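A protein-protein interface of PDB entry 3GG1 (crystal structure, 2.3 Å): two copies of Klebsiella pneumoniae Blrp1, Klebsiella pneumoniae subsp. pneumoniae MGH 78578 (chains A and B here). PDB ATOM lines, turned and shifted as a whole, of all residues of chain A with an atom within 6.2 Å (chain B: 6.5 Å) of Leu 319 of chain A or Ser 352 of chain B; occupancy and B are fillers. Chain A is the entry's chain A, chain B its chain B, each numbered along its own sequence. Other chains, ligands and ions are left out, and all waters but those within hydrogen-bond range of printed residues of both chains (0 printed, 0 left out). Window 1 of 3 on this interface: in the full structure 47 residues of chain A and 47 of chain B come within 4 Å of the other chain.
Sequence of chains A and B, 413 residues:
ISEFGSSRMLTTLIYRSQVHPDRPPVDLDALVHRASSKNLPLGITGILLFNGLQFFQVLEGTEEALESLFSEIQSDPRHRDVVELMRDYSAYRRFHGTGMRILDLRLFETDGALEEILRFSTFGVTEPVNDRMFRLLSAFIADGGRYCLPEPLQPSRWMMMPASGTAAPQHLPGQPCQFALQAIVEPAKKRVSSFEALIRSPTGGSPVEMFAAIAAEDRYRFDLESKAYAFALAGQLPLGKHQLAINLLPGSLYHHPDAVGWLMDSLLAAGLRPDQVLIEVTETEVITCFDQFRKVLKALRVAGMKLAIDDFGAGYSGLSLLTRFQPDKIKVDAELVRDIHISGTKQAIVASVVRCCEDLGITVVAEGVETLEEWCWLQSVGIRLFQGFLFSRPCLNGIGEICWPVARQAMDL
Ser 317 of chain A touches Gly 318 of chain B. N of Gly 318 of chain A touches O of Ser 317 of chain B (3.7 Å). Gly 318 of chain A touches Gly 318 of chain B. CD1 of Leu 319 of chain B touches CD1 of Leu 319 of chain A, at 3.9 Å. Ser 352 of chain B touches Leu 319 of chain A (OG to CD1, 3.9 Å). Thr 323 of chain A touches Leu 336 of chain B. Ile 349 of chain B touches Thr 323 of chain A (CD1 to CG2, 3.6 Å). Cys 356 of chain B touches Ser 352 of chain A. Arg 355 of chain B touches Arg 355 of chain A. Cys 356 of chain A touches Ser 352 of chain B.
Of the printed residues of chain B, Gly 318 of chain A touches Ser 317 and Gly 318. Of chain B, only Leu 319 (3.9 Å), Ile 349 (3.2 Å) and Ser 352 (3.9 Å) come within 4 Å of Leu 319 of chain A. Val 354 of chain A touches none of the printed residues of chain B. Of the printed residues of chain A, Leu 319 of chain B touches Leu 319 (3.9 Å) and Ser 352 (3.2 Å). Of the printed residues of chain A, Ile 349 of chain B touches Leu 319, Thr 323 and Cys 356. Ser 352 of chain B touches just these residues of chain A: Leu 319 (3.9 Å), Ser 352 (2.5 Å) and Cys 356 (3.8 Å). The nearest printed residue of chain A that does not touch Ser 317 of chain B is Ser 317 of chain A (4.2 Å).
Of the 18 printed residues of chain B, 10 touch a printed residue of chain A. Printed residues of chain A that touch a printed residue of chain B: Ser 317, Gly 318, Leu 319, Ser 320, Leu 322, Thr 323, Ser 352, Arg 355 and Cys 356. Among the printed residues, no Asp or Glu carboxylate lies within 4 Å of a Lys or Arg side-chain nitrogen of the other chain.
O of Ser 317 of chain B lies within hydrogen-bond range of OG of Ser 320 of chain A (2.7 Å). The backbone carbonyl oxygen (O) of Ser 352 of chain A sits at hydrogen-bond distance from the side-chain hydroxyl (OG) of Ser 352 of chain B (2.5 Å).
O of Ser 320 of chain A lies within hydrogen-bond range of OG1 of Thr 323 of chain A, at 2.7 Å. O of Ala 351 of chain A lies close to NH1 of Arg 355 of chain A (3.5 Å).
Ser 317 of chain A touches Gly 318 of chain B, and with the chains exchanged Gly 318 of chain A touches Ser 317 of chain B. Gly 318 of chain A touches its own counterpart, Gly 318 of chain B. Leu 319 of chain A touches its own counterpart, Leu 319 of chain B. Ser 352 of chain A touches Cys 356 of chain B, and with the chains exchanged Cys 356 of chain A touches Ser 352 of chain B. Positions printed for both chains: 317, 318, 319, 351, 352, 353, 354, 355, 356 and 357. Of the 17 pairs that touch across the chains among the printed residues, 10 have their exchanged pair printed and touching as well.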
ATOM      1  N   PHE A 312     -10.772  22.190 -25.513  1.00  0.00           N
ATOM      2  CA  PHE A 312     -12.213  22.082 -25.334  1.00  0.00           C
ATOM      3  C   PHE A 312     -12.518  21.481 -23.963  1.00  0.00           C
ATOM      4  O   PHE A 312     -12.060  20.385 -23.643  1.00  0.00           O
ATOM      5  CB  PHE A 312     -12.829  21.231 -26.444  1.00  0.00           C
ATOM      6  CG  PHE A 312     -14.329  21.282 -26.483  1.00  0.00           C
ATOM      7  CD1 PHE A 312     -14.985  22.312 -27.143  1.00  0.00           C
ATOM      8  CD2 PHE A 312     -15.087  20.300 -25.862  1.00  0.00           C
ATOM      9  CE1 PHE A 312     -16.372  22.365 -27.180  1.00  0.00           C
ATOM     10  CE2 PHE A 312     -16.474  20.347 -25.896  1.00  0.00           C
ATOM     11  CZ  PHE A 312     -17.117  21.380 -26.558  1.00  0.00           C
ATOM     12  N   SER A 317     -17.563  26.585 -21.834  1.00  0.00           N
ATOM     13  CA  SER A 317     -16.724  25.742 -22.709  1.00  0.00           C
ATOM     14  C   SER A 317     -17.554  25.254 -23.886  1.00  0.00           C
ATOM     15  O   SER A 317     -17.257  25.525 -25.049  1.00  0.00           O
ATOM     16  CB  SER A 317     -16.181  24.469 -22.035  1.00  0.00           C
ATOM     17  OG  SER A 317     -17.194  23.778 -21.328  1.00  0.00           O
ATOM     18  N   GLY A 318     -18.635  24.570 -23.538  1.00  0.00           N
ATOM     19  CA  GLY A 318     -19.041  23.365 -24.226  1.00  0.00           C
ATOM     20  C   GLY A 318     -19.843  23.432 -25.501  1.00  0.00           C
ATOM     21  O   GLY A 318     -19.609  24.268 -26.374  1.00  0.00           O
ATOM     22  N   LEU A 319     -20.806  22.521 -25.579  1.00  0.00           N
ATOM     23  CA  LEU A 319     -21.425  22.115 -26.833  1.00  0.00           C
ATOM     24  C   LEU A 319     -22.354  23.172 -27.412  1.00  0.00           C
ATOM     25  O   LEU A 319     -22.643  23.150 -28.605  1.00  0.00           O
ATOM     26  CB  LEU A 319     -22.181  20.797 -26.624  1.00  0.00           C
ATOM     27  CG  LEU A 319     -21.330  19.625 -26.117  1.00  0.00           C
ATOM     28  CD1 LEU A 319     -22.207  18.487 -25.628  1.00  0.00           C
ATOM     29  CD2 LEU A 319     -20.367  19.145 -27.198  1.00  0.00           C
ATOM     30  N   SER A 320     -22.815  24.092 -26.568  1.00  0.00           N
ATOM     31  CA  SER A 320     -23.637  25.219 -27.007  1.00  0.00           C
ATOM     32  C   SER A 320     -22.945  26.070 -28.076  1.00  0.00           C
ATOM     33  O   SER A 320     -23.608  26.645 -28.935  1.00  0.00           O
ATOM     34  CB  SER A 320     -24.016  26.090 -25.810  1.00  0.00           C
ATOM     35  OG  SER A 320     -22.898  26.311 -24.962  1.00  0.00           O
ATOM     36  N   LEU A 321     -21.616  26.142 -28.016  1.00  0.00           N
ATOM     37  CA  LEU A 321     -20.818  26.791 -29.062  1.00  0.00           C
ATOM     38  C   LEU A 321     -21.081  26.213 -30.463  1.00  0.00           C
ATOM     39  O   LEU A 321     -20.940  26.915 -31.463  1.00  0.00           O
ATOM     40  CB  LEU A 321     -19.325  26.676 -28.727  1.00  0.00           C
ATOM     41  CG  LEU A 321     -18.299  27.175 -29.754  1.00  0.00           C
ATOM     42  CD1 LEU A 321     -18.608  28.585 -30.203  1.00  0.00           C
ATOM     43  CD2 LEU A 321     -16.895  27.111 -29.182  1.00  0.00           C
ATOM     44  N   LEU A 322     -21.473  24.941 -30.529  1.00  0.00           N
ATOM     45  CA  LEU A 322     -21.678  24.264 -31.810  1.00  0.00           C
ATOM     46  C   LEU A 322     -22.894  24.776 -32.583  1.00  0.00           C
ATOM     47  O   LEU A 322     -23.006  24.534 -33.781  1.00  0.00           O
ATOM     48  CB  LEU A 322     -21.766  22.746 -31.617  1.00  0.00           C
ATOM     49  CG  LEU A 322     -20.543  22.128 -30.930  1.00  0.00           C
ATOM     50  CD1 LEU A 322     -20.761  20.651 -30.650  1.00  0.00           C
ATOM     51  CD2 LEU A 322     -19.283  22.344 -31.767  1.00  0.00           C
ATOM     52  N   THR A 323     -23.792  25.498 -31.917  1.00  0.00           N
ATOM     53  CA  THR A 323     -24.897  26.151 -32.614  1.00  0.00           C
ATOM     54  C   THR A 323     -24.436  27.367 -33.424  1.00  0.00           C
ATOM     55  O   THR A 323     -25.235  27.957 -34.155  1.00  0.00           O
ATOM     56  CB  THR A 323     -25.996  26.636 -31.632  1.00  0.00           C
ATOM     57  OG1 THR A 323     -25.435  27.555 -30.684  1.00  0.00           O
ATOM     58  CG2 THR A 323     -26.633  25.463 -30.896  1.00  0.00           C
ATOM     59  N   ALA A 351     -17.512  11.298 -22.710  1.00  0.00           N
ATOM     60  CA  ALA A 351     -18.437  10.464 -23.486  1.00  0.00           C
ATOM     61  C   ALA A 351     -19.512  11.295 -24.195  1.00  0.00           C
ATOM     62  O   ALA A 351     -19.913  10.970 -25.315  1.00  0.00           O
ATOM     63  CB  ALA A 351     -19.084   9.412 -22.595  1.00  0.00           C
ATOM     64  N   SER A 352     -19.971  12.365 -23.548  1.00  0.00           N
ATOM     65  CA  SER A 352     -20.996  13.233 -24.134  1.00  0.00           C
ATOM     66  C   SER A 352     -20.430  14.057 -25.299  1.00  0.00           C
ATOM     67  O   SER A 352     -21.105  14.253 -26.313  1.00  0.00           O
ATOM     68  CB  SER A 352     -21.624  14.143 -23.064  1.00  0.00           C
ATOM     69  OG  SER A 352     -20.697  15.099 -22.579  1.00  0.00           O
ATOM     70  N   VAL A 353     -19.190  14.517 -25.157  1.00  0.00           N
ATOM     71  CA  VAL A 353     -18.499  15.231 -26.231  1.00  0.00           C
ATOM     72  C   VAL A 353     -18.285  14.321 -27.451  1.00  0.00           C
ATOM     73  O   VAL A 353     -18.503  14.739 -28.592  1.00  0.00           O
ATOM     74  CB  VAL A 353     -17.135  15.802 -25.751  1.00  0.00           C
ATOM     75  CG1 VAL A 353     -16.345  16.379 -26.916  1.00  0.00           C
ATOM     76  CG2 VAL A 353     -17.348  16.870 -24.696  1.00  0.00           C
ATOM     77  N   VAL A 354     -17.853  13.085 -27.196  1.00  0.00           N
ATOM     78  CA  VAL A 354     -17.660  12.089 -28.253  1.00  0.00           C
ATOM     79  C   VAL A 354     -18.959  11.851 -29.019  1.00  0.00           C
ATOM     80  O   VAL A 354     -18.983  11.901 -30.244  1.00  0.00           O
ATOM     81  CB  VAL A 354     -17.145  10.744 -27.673  1.00  0.00           C
ATOM     82  CG1 VAL A 354     -17.290   9.601 -28.685  1.00  0.00           C
ATOM     83  CG2 VAL A 354     -15.701  10.876 -27.246  1.00  0.00           C
ATOM     84  N   ARG A 355     -20.034  11.613 -28.276  1.00  0.00           N
ATOM     85  CA  ARG A 355     -21.328  11.273 -28.861  1.00  0.00           C
ATOM     86  C   ARG A 355     -21.935  12.445 -29.644  1.00  0.00           C
ATOM     87  O   ARG A 355     -22.496  12.250 -30.722  1.00  0.00           O
ATOM     88  CB  ARG A 355     -22.277  10.811 -27.759  1.00  0.00           C
ATOM     89  CG  ARG A 355     -23.324   9.806 -28.189  1.00  0.00           C
ATOM     90  CD  ARG A 355     -23.889   9.071 -26.978  1.00  0.00           C
ATOM     91  NE  ARG A 355     -24.006   9.976 -25.831  1.00  0.00           N
ATOM     92  CZ  ARG A 355     -23.352   9.862 -24.674  1.00  0.00           C
ATOM     93  NH1 ARG A 355     -22.532   8.840 -24.421  1.00  0.00           N
ATOM     94  NH2 ARG A 355     -23.545  10.781 -23.744  1.00  0.00           N
ATOM     95  N   CYS A 356     -21.804  13.657 -29.108  1.00  0.00           N
ATOM     96  CA  CYS A 356     -22.263  14.862 -29.807  1.00  0.00           C
ATOM     97  C   CYS A 356     -21.499  15.106 -31.115  1.00  0.00           C
ATOM     98  O   CYS A 356     -22.098  15.357 -32.155  1.00  0.00           O
ATOM     99  CB  CYS A 356     -22.143  16.090 -28.908  1.00  0.00           C
ATOM    100  SG  CYS A 356     -22.916  17.560 -29.618  1.00  0.00           S
ATOM    101  N   CYS A 357     -20.176  15.025 -31.050  1.00  0.00           N
ATOM    102  CA  CYS A 357     -19.326  15.220 -32.225  1.00  0.00           C
ATOM    103  C   CYS A 357     -19.538  14.145 -33.291  1.00  0.00           C
ATOM    104  O   CYS A 357     -19.499  14.435 -34.487  1.00  0.00           O
ATOM    105  CB  CYS A 357     -17.861  15.255 -31.806  1.00  0.00           C
ATOM    106  SG  CYS A 357     -17.446  16.714 -30.862  1.00  0.00           S
ATOM    107  N   TYR B 147     -31.667   9.164 -34.720  1.00  0.00           N
ATOM    108  CA  TYR B 147     -32.533  10.332 -34.525  1.00  0.00           C
ATOM    109  C   TYR B 147     -33.811  10.250 -35.353  1.00  0.00           C
ATOM    110  O   TYR B 147     -34.445  11.267 -35.646  1.00  0.00           O
ATOM    111  CB  TYR B 147     -31.768  11.627 -34.806  1.00  0.00           C
ATOM    112  CG  TYR B 147     -30.765  11.927 -33.730  1.00  0.00           C
ATOM    113  CD1 TYR B 147     -31.116  12.693 -32.620  1.00  0.00           C
ATOM    114  CD2 TYR B 147     -29.474  11.418 -33.796  1.00  0.00           C
ATOM    115  CE1 TYR B 147     -30.198  12.958 -31.614  1.00  0.00           C
ATOM    116  CE2 TYR B 147     -28.554  11.678 -32.798  1.00  0.00           C
ATOM    117  CZ  TYR B 147     -28.921  12.450 -31.709  1.00  0.00           C
ATOM    118  OH  TYR B 147     -28.010  12.712 -30.713  1.00  0.00           O
ATOM    119  N   SER B 317     -21.448  28.093 -21.739  1.00  0.00           N
ATOM    120  CA  SER B 317     -22.228  27.090 -21.039  1.00  0.00           C
ATOM    121  C   SER B 317     -21.813  25.697 -21.473  1.00  0.00           C
ATOM    122  O   SER B 317     -22.144  25.271 -22.584  1.00  0.00           O
ATOM    123  CB  SER B 317     -23.708  27.287 -21.375  1.00  0.00           C
ATOM    124  OG  SER B 317     -24.308  28.267 -20.542  1.00  0.00           O
ATOM    125  N   GLY B 318     -21.102  24.988 -20.599  1.00  0.00           N
ATOM    126  CA  GLY B 318     -20.611  23.653 -20.926  1.00  0.00           C
ATOM    127  C   GLY B 318     -20.699  22.643 -19.806  1.00  0.00           C
ATOM    128  O   GLY B 318     -20.997  22.982 -18.662  1.00  0.00           O
ATOM    129  N   LEU B 319     -20.417  21.392 -20.154  1.00  0.00           N
ATOM    130  CA  LEU B 319     -20.453  20.283 -19.209  1.00  0.00           C
ATOM    131  C   LEU B 319     -19.144  20.157 -18.423  1.00  0.00           C
ATOM    132  O   LEU B 319     -19.118  19.517 -17.377  1.00  0.00           O
ATOM    133  CB  LEU B 319     -20.750  18.974 -19.947  1.00  0.00           C
ATOM    134  CG  LEU B 319     -22.091  18.920 -20.691  1.00  0.00           C
ATOM    135  CD1 LEU B 319     -22.093  17.817 -21.737  1.00  0.00           C
ATOM    136  CD2 LEU B 319     -23.246  18.732 -19.718  1.00  0.00           C
ATOM    137  N   LEU B 336     -31.888  26.469 -27.042  1.00  0.00           N
ATOM    138  CA  LEU B 336     -31.624  25.119 -27.550  1.00  0.00           C
ATOM    139  C   LEU B 336     -32.928  24.396 -27.873  1.00  0.00           C
ATOM    140  O   LEU B 336     -32.953  23.508 -28.724  1.00  0.00           O
ATOM    141  CB  LEU B 336     -30.809  24.300 -26.544  1.00  0.00           C
ATOM    142  CG  LEU B 336     -29.321  24.632 -26.437  1.00  0.00           C
ATOM    143  CD1 LEU B 336     -28.694  23.850 -25.290  1.00  0.00           C
ATOM    144  CD2 LEU B 336     -28.590  24.342 -27.748  1.00  0.00           C
ATOM    145  N   THR B 345     -28.153  19.903 -35.045  1.00  0.00           N
ATOM    146  CA  THR B 345     -27.174  20.412 -34.089  1.00  0.00           C
ATOM    147  C   THR B 345     -27.757  20.499 -32.680  1.00  0.00           C
ATOM    148  O   THR B 345     -27.165  19.987 -31.730  1.00  0.00           O
ATOM    149  CB  THR B 345     -26.645  21.790 -34.522  1.00  0.00           C
ATOM    150  OG1 THR B 345     -26.258  21.738 -35.899  1.00  0.00           O
ATOM    151  CG2 THR B 345     -25.443  22.199 -33.690  1.00  0.00           C
ATOM    152  N   GLN B 347     -30.501  18.996 -31.635  1.00  0.00           N
ATOM    153  CA  GLN B 347     -30.835  17.614 -31.266  1.00  0.00           C
ATOM    154  C   GLN B 347     -29.643  16.876 -30.654  1.00  0.00           C
ATOM    155  O   GLN B 347     -29.768  16.248 -29.603  1.00  0.00           O
ATOM    156  CB  GLN B 347     -31.358  16.840 -32.482  1.00  0.00           C
ATOM    157  CG  GLN B 347     -32.775  17.221 -32.878  1.00  0.00           C
ATOM    158  CD  GLN B 347     -33.208  16.631 -34.209  1.00  0.00           C
ATOM    159  OE1 GLN B 347     -32.611  15.675 -34.701  1.00  0.00           O
ATOM    160  NE2 GLN B 347     -34.259  17.198 -34.795  1.00  0.00           N
ATOM    161  N   ALA B 348     -28.490  16.970 -31.311  1.00  0.00           N
ATOM    162  CA  ALA B 348     -27.271  16.306 -30.852  1.00  0.00           C
ATOM    163  C   ALA B 348     -26.759  16.863 -29.517  1.00  0.00           C
ATOM    164  O   ALA B 348     -26.318  16.105 -28.658  1.00  0.00           O
ATOM    165  CB  ALA B 348     -26.190  16.411 -31.913  1.00  0.00           C
ATOM    166  N   ILE B 349     -26.819  18.183 -29.357  1.00  0.00           N
ATOM    167  CA  ILE B 349     -26.380  18.848 -28.127  1.00  0.00           C
ATOM    168  C   ILE B 349     -27.289  18.487 -26.955  1.00  0.00           C
ATOM    169  O   ILE B 349     -26.811  18.107 -25.888  1.00  0.00           O
ATOM    170  CB  ILE B 349     -26.347  20.392 -28.291  1.00  0.00           C
ATOM    171  CG1 ILE B 349     -25.252  20.801 -29.281  1.00  0.00           C
ATOM    172  CG2 ILE B 349     -26.122  21.086 -26.940  1.00  0.00           C
ATOM    173  CD1 ILE B 349     -25.424  22.196 -29.836  1.00  0.00           C
ATOM    174  N   VAL B 350     -28.597  18.604 -27.163  1.00  0.00           N
ATOM    175  CA  VAL B 350     -29.572  18.341 -26.107  1.00  0.00           C
ATOM    176  C   VAL B 350     -29.559  16.858 -25.712  1.00  0.00           C
ATOM    177  O   VAL B 350     -29.581  16.533 -24.527  1.00  0.00           O
ATOM    178  CB  VAL B 350     -30.996  18.791 -26.518  1.00  0.00           C
ATOM    179  CG1 VAL B 350     -32.025  18.379 -25.463  1.00  0.00           C
ATOM    180  CG2 VAL B 350     -31.040  20.305 -26.732  1.00  0.00           C
ATOM    181  N   ALA B 351     -29.510  15.970 -26.703  1.00  0.00           N
ATOM    182  CA  ALA B 351     -29.378  14.527 -26.451  1.00  0.00           C
ATOM    183  C   ALA B 351     -28.133  14.203 -25.623  1.00  0.00           C
ATOM    184  O   ALA B 351     -28.154  13.314 -24.774  1.00  0.00           O
ATOM    185  CB  ALA B 351     -29.339  13.761 -27.767  1.00  0.00           C
ATOM    186  N   SER B 352     -27.057  14.945 -25.870  1.00  0.00           N
ATOM    187  CA  SER B 352     -25.789  14.725 -25.183  1.00  0.00           C
ATOM    188  C   SER B 352     -25.809  15.242 -23.748  1.00  0.00           C
ATOM    189  O   SER B 352     -25.251  14.607 -22.851  1.00  0.00           O
ATOM    190  CB  SER B 352     -24.651  15.380 -25.962  1.00  0.00           C
ATOM    191  OG  SER B 352     -23.423  14.792 -25.607  1.00  0.00           O
ATOM    192  N   VAL B 353     -26.442  16.395 -23.539  1.00  0.00           N
ATOM    193  CA  VAL B 353     -26.636  16.955 -22.195  1.00  0.00           C
ATOM    194  C   VAL B 353     -27.514  16.040 -21.336  1.00  0.00           C
ATOM    195  O   VAL B 353     -27.201  15.790 -20.170  1.00  0.00           O
ATOM    196  CB  VAL B 353     -27.277  18.374 -22.256  1.00  0.00           C
ATOM    197  CG1 VAL B 353     -27.762  18.828 -20.877  1.00  0.00           C
ATOM    198  CG2 VAL B 353     -26.283  19.380 -22.825  1.00  0.00           C
ATOM    199  N   VAL B 354     -28.610  15.557 -21.916  1.00  0.00           N
ATOM    200  CA  VAL B 354     -29.525  14.649 -21.221  1.00  0.00           C
ATOM    201  C   VAL B 354     -28.779  13.414 -20.705  1.00  0.00           C
ATOM    202  O   VAL B 354     -28.945  13.007 -19.555  1.00  0.00           O
ATOM    203  CB  VAL B 354     -30.693  14.210 -22.147  1.00  0.00           C
ATOM    204  CG1 VAL B 354     -31.417  12.986 -21.594  1.00  0.00           C
ATOM    205  CG2 VAL B 354     -31.667  15.359 -22.347  1.00  0.00           C
ATOM    206  N   ARG B 355     -27.950  12.836 -21.567  1.00  0.00           N
ATOM    207  CA  ARG B 355     -27.240  11.611 -21.241  1.00  0.00           C
ATOM    208  C   ARG B 355     -26.190  11.837 -20.159  1.00  0.00           C
ATOM    209  O   ARG B 355     -26.065  11.032 -19.234  1.00  0.00           O
ATOM    210  CB  ARG B 355     -26.574  11.057 -22.491  1.00  0.00           C
ATOM    211  CG  ARG B 355     -26.090   9.639 -22.349  1.00  0.00           C
ATOM    212  CD  ARG B 355     -27.235   8.667 -22.290  1.00  0.00           C
ATOM    213  NE  ARG B 355     -26.845   7.373 -22.845  1.00  0.00           N
ATOM    214  CZ  ARG B 355     -27.696   6.426 -23.230  1.00  0.00           C
ATOM    215  NH1 ARG B 355     -29.015   6.602 -23.133  1.00  0.00           N
ATOM    216  NH2 ARG B 355     -27.220   5.291 -23.725  1.00  0.00           N
ATOM    217  N   CYS B 356     -25.431  12.922 -20.291  1.00  0.00           N
ATOM    218  CA  CYS B 356     -24.431  13.294 -19.298  1.00  0.00           C
ATOM    219  C   CYS B 356     -25.070  13.485 -17.922  1.00  0.00           C
ATOM    220  O   CYS B 356     -24.559  12.988 -16.920  1.00  0.00           O
ATOM    221  CB  CYS B 356     -23.709  14.572 -19.723  1.00  0.00           C
ATOM    222  SG  CYS B 356     -22.304  15.011 -18.685  1.00  0.00           S
ATOM    223  N   CYS B 357     -26.192  14.196 -17.888  1.00  0.00           N
ATOM    224  CA  CYS B 357     -26.936  14.417 -16.648  1.00  0.00           C
ATOM    225  C   CYS B 357     -27.459  13.121 -16.024  1.00  0.00           C
ATOM    226  O   CYS B 357     -27.462  12.983 -14.801  1.00  0.00           O
ATOM    227  CB  CYS B 357     -28.098  15.377 -16.890  1.00  0.00           C
ATOM    228  SG  CYS B 357     -27.578  17.068 -17.158  1.00  0.00           S
ATOM    229  N   VAL B 381     -35.245  12.568 -27.229  1.00  0.00           N
ATOM    230  CA  VAL B 381     -33.848  12.559 -26.770  1.00  0.00           C
ATOM    231  C   VAL B 381     -33.704  12.434 -25.238  1.00  0.00           C
ATOM    232  O   VAL B 381     -32.620  12.664 -24.694  1.00  0.00           O
ATOM    233  CB  VAL B 381     -33.061  13.803 -27.283  1.00  0.00           C
ATOM    234  CG1 VAL B 381     -33.074  13.851 -28.809  1.00  0.00           C
ATOM    235  CG2 VAL B 381     -33.610  15.107 -26.699  1.00  0.00           C
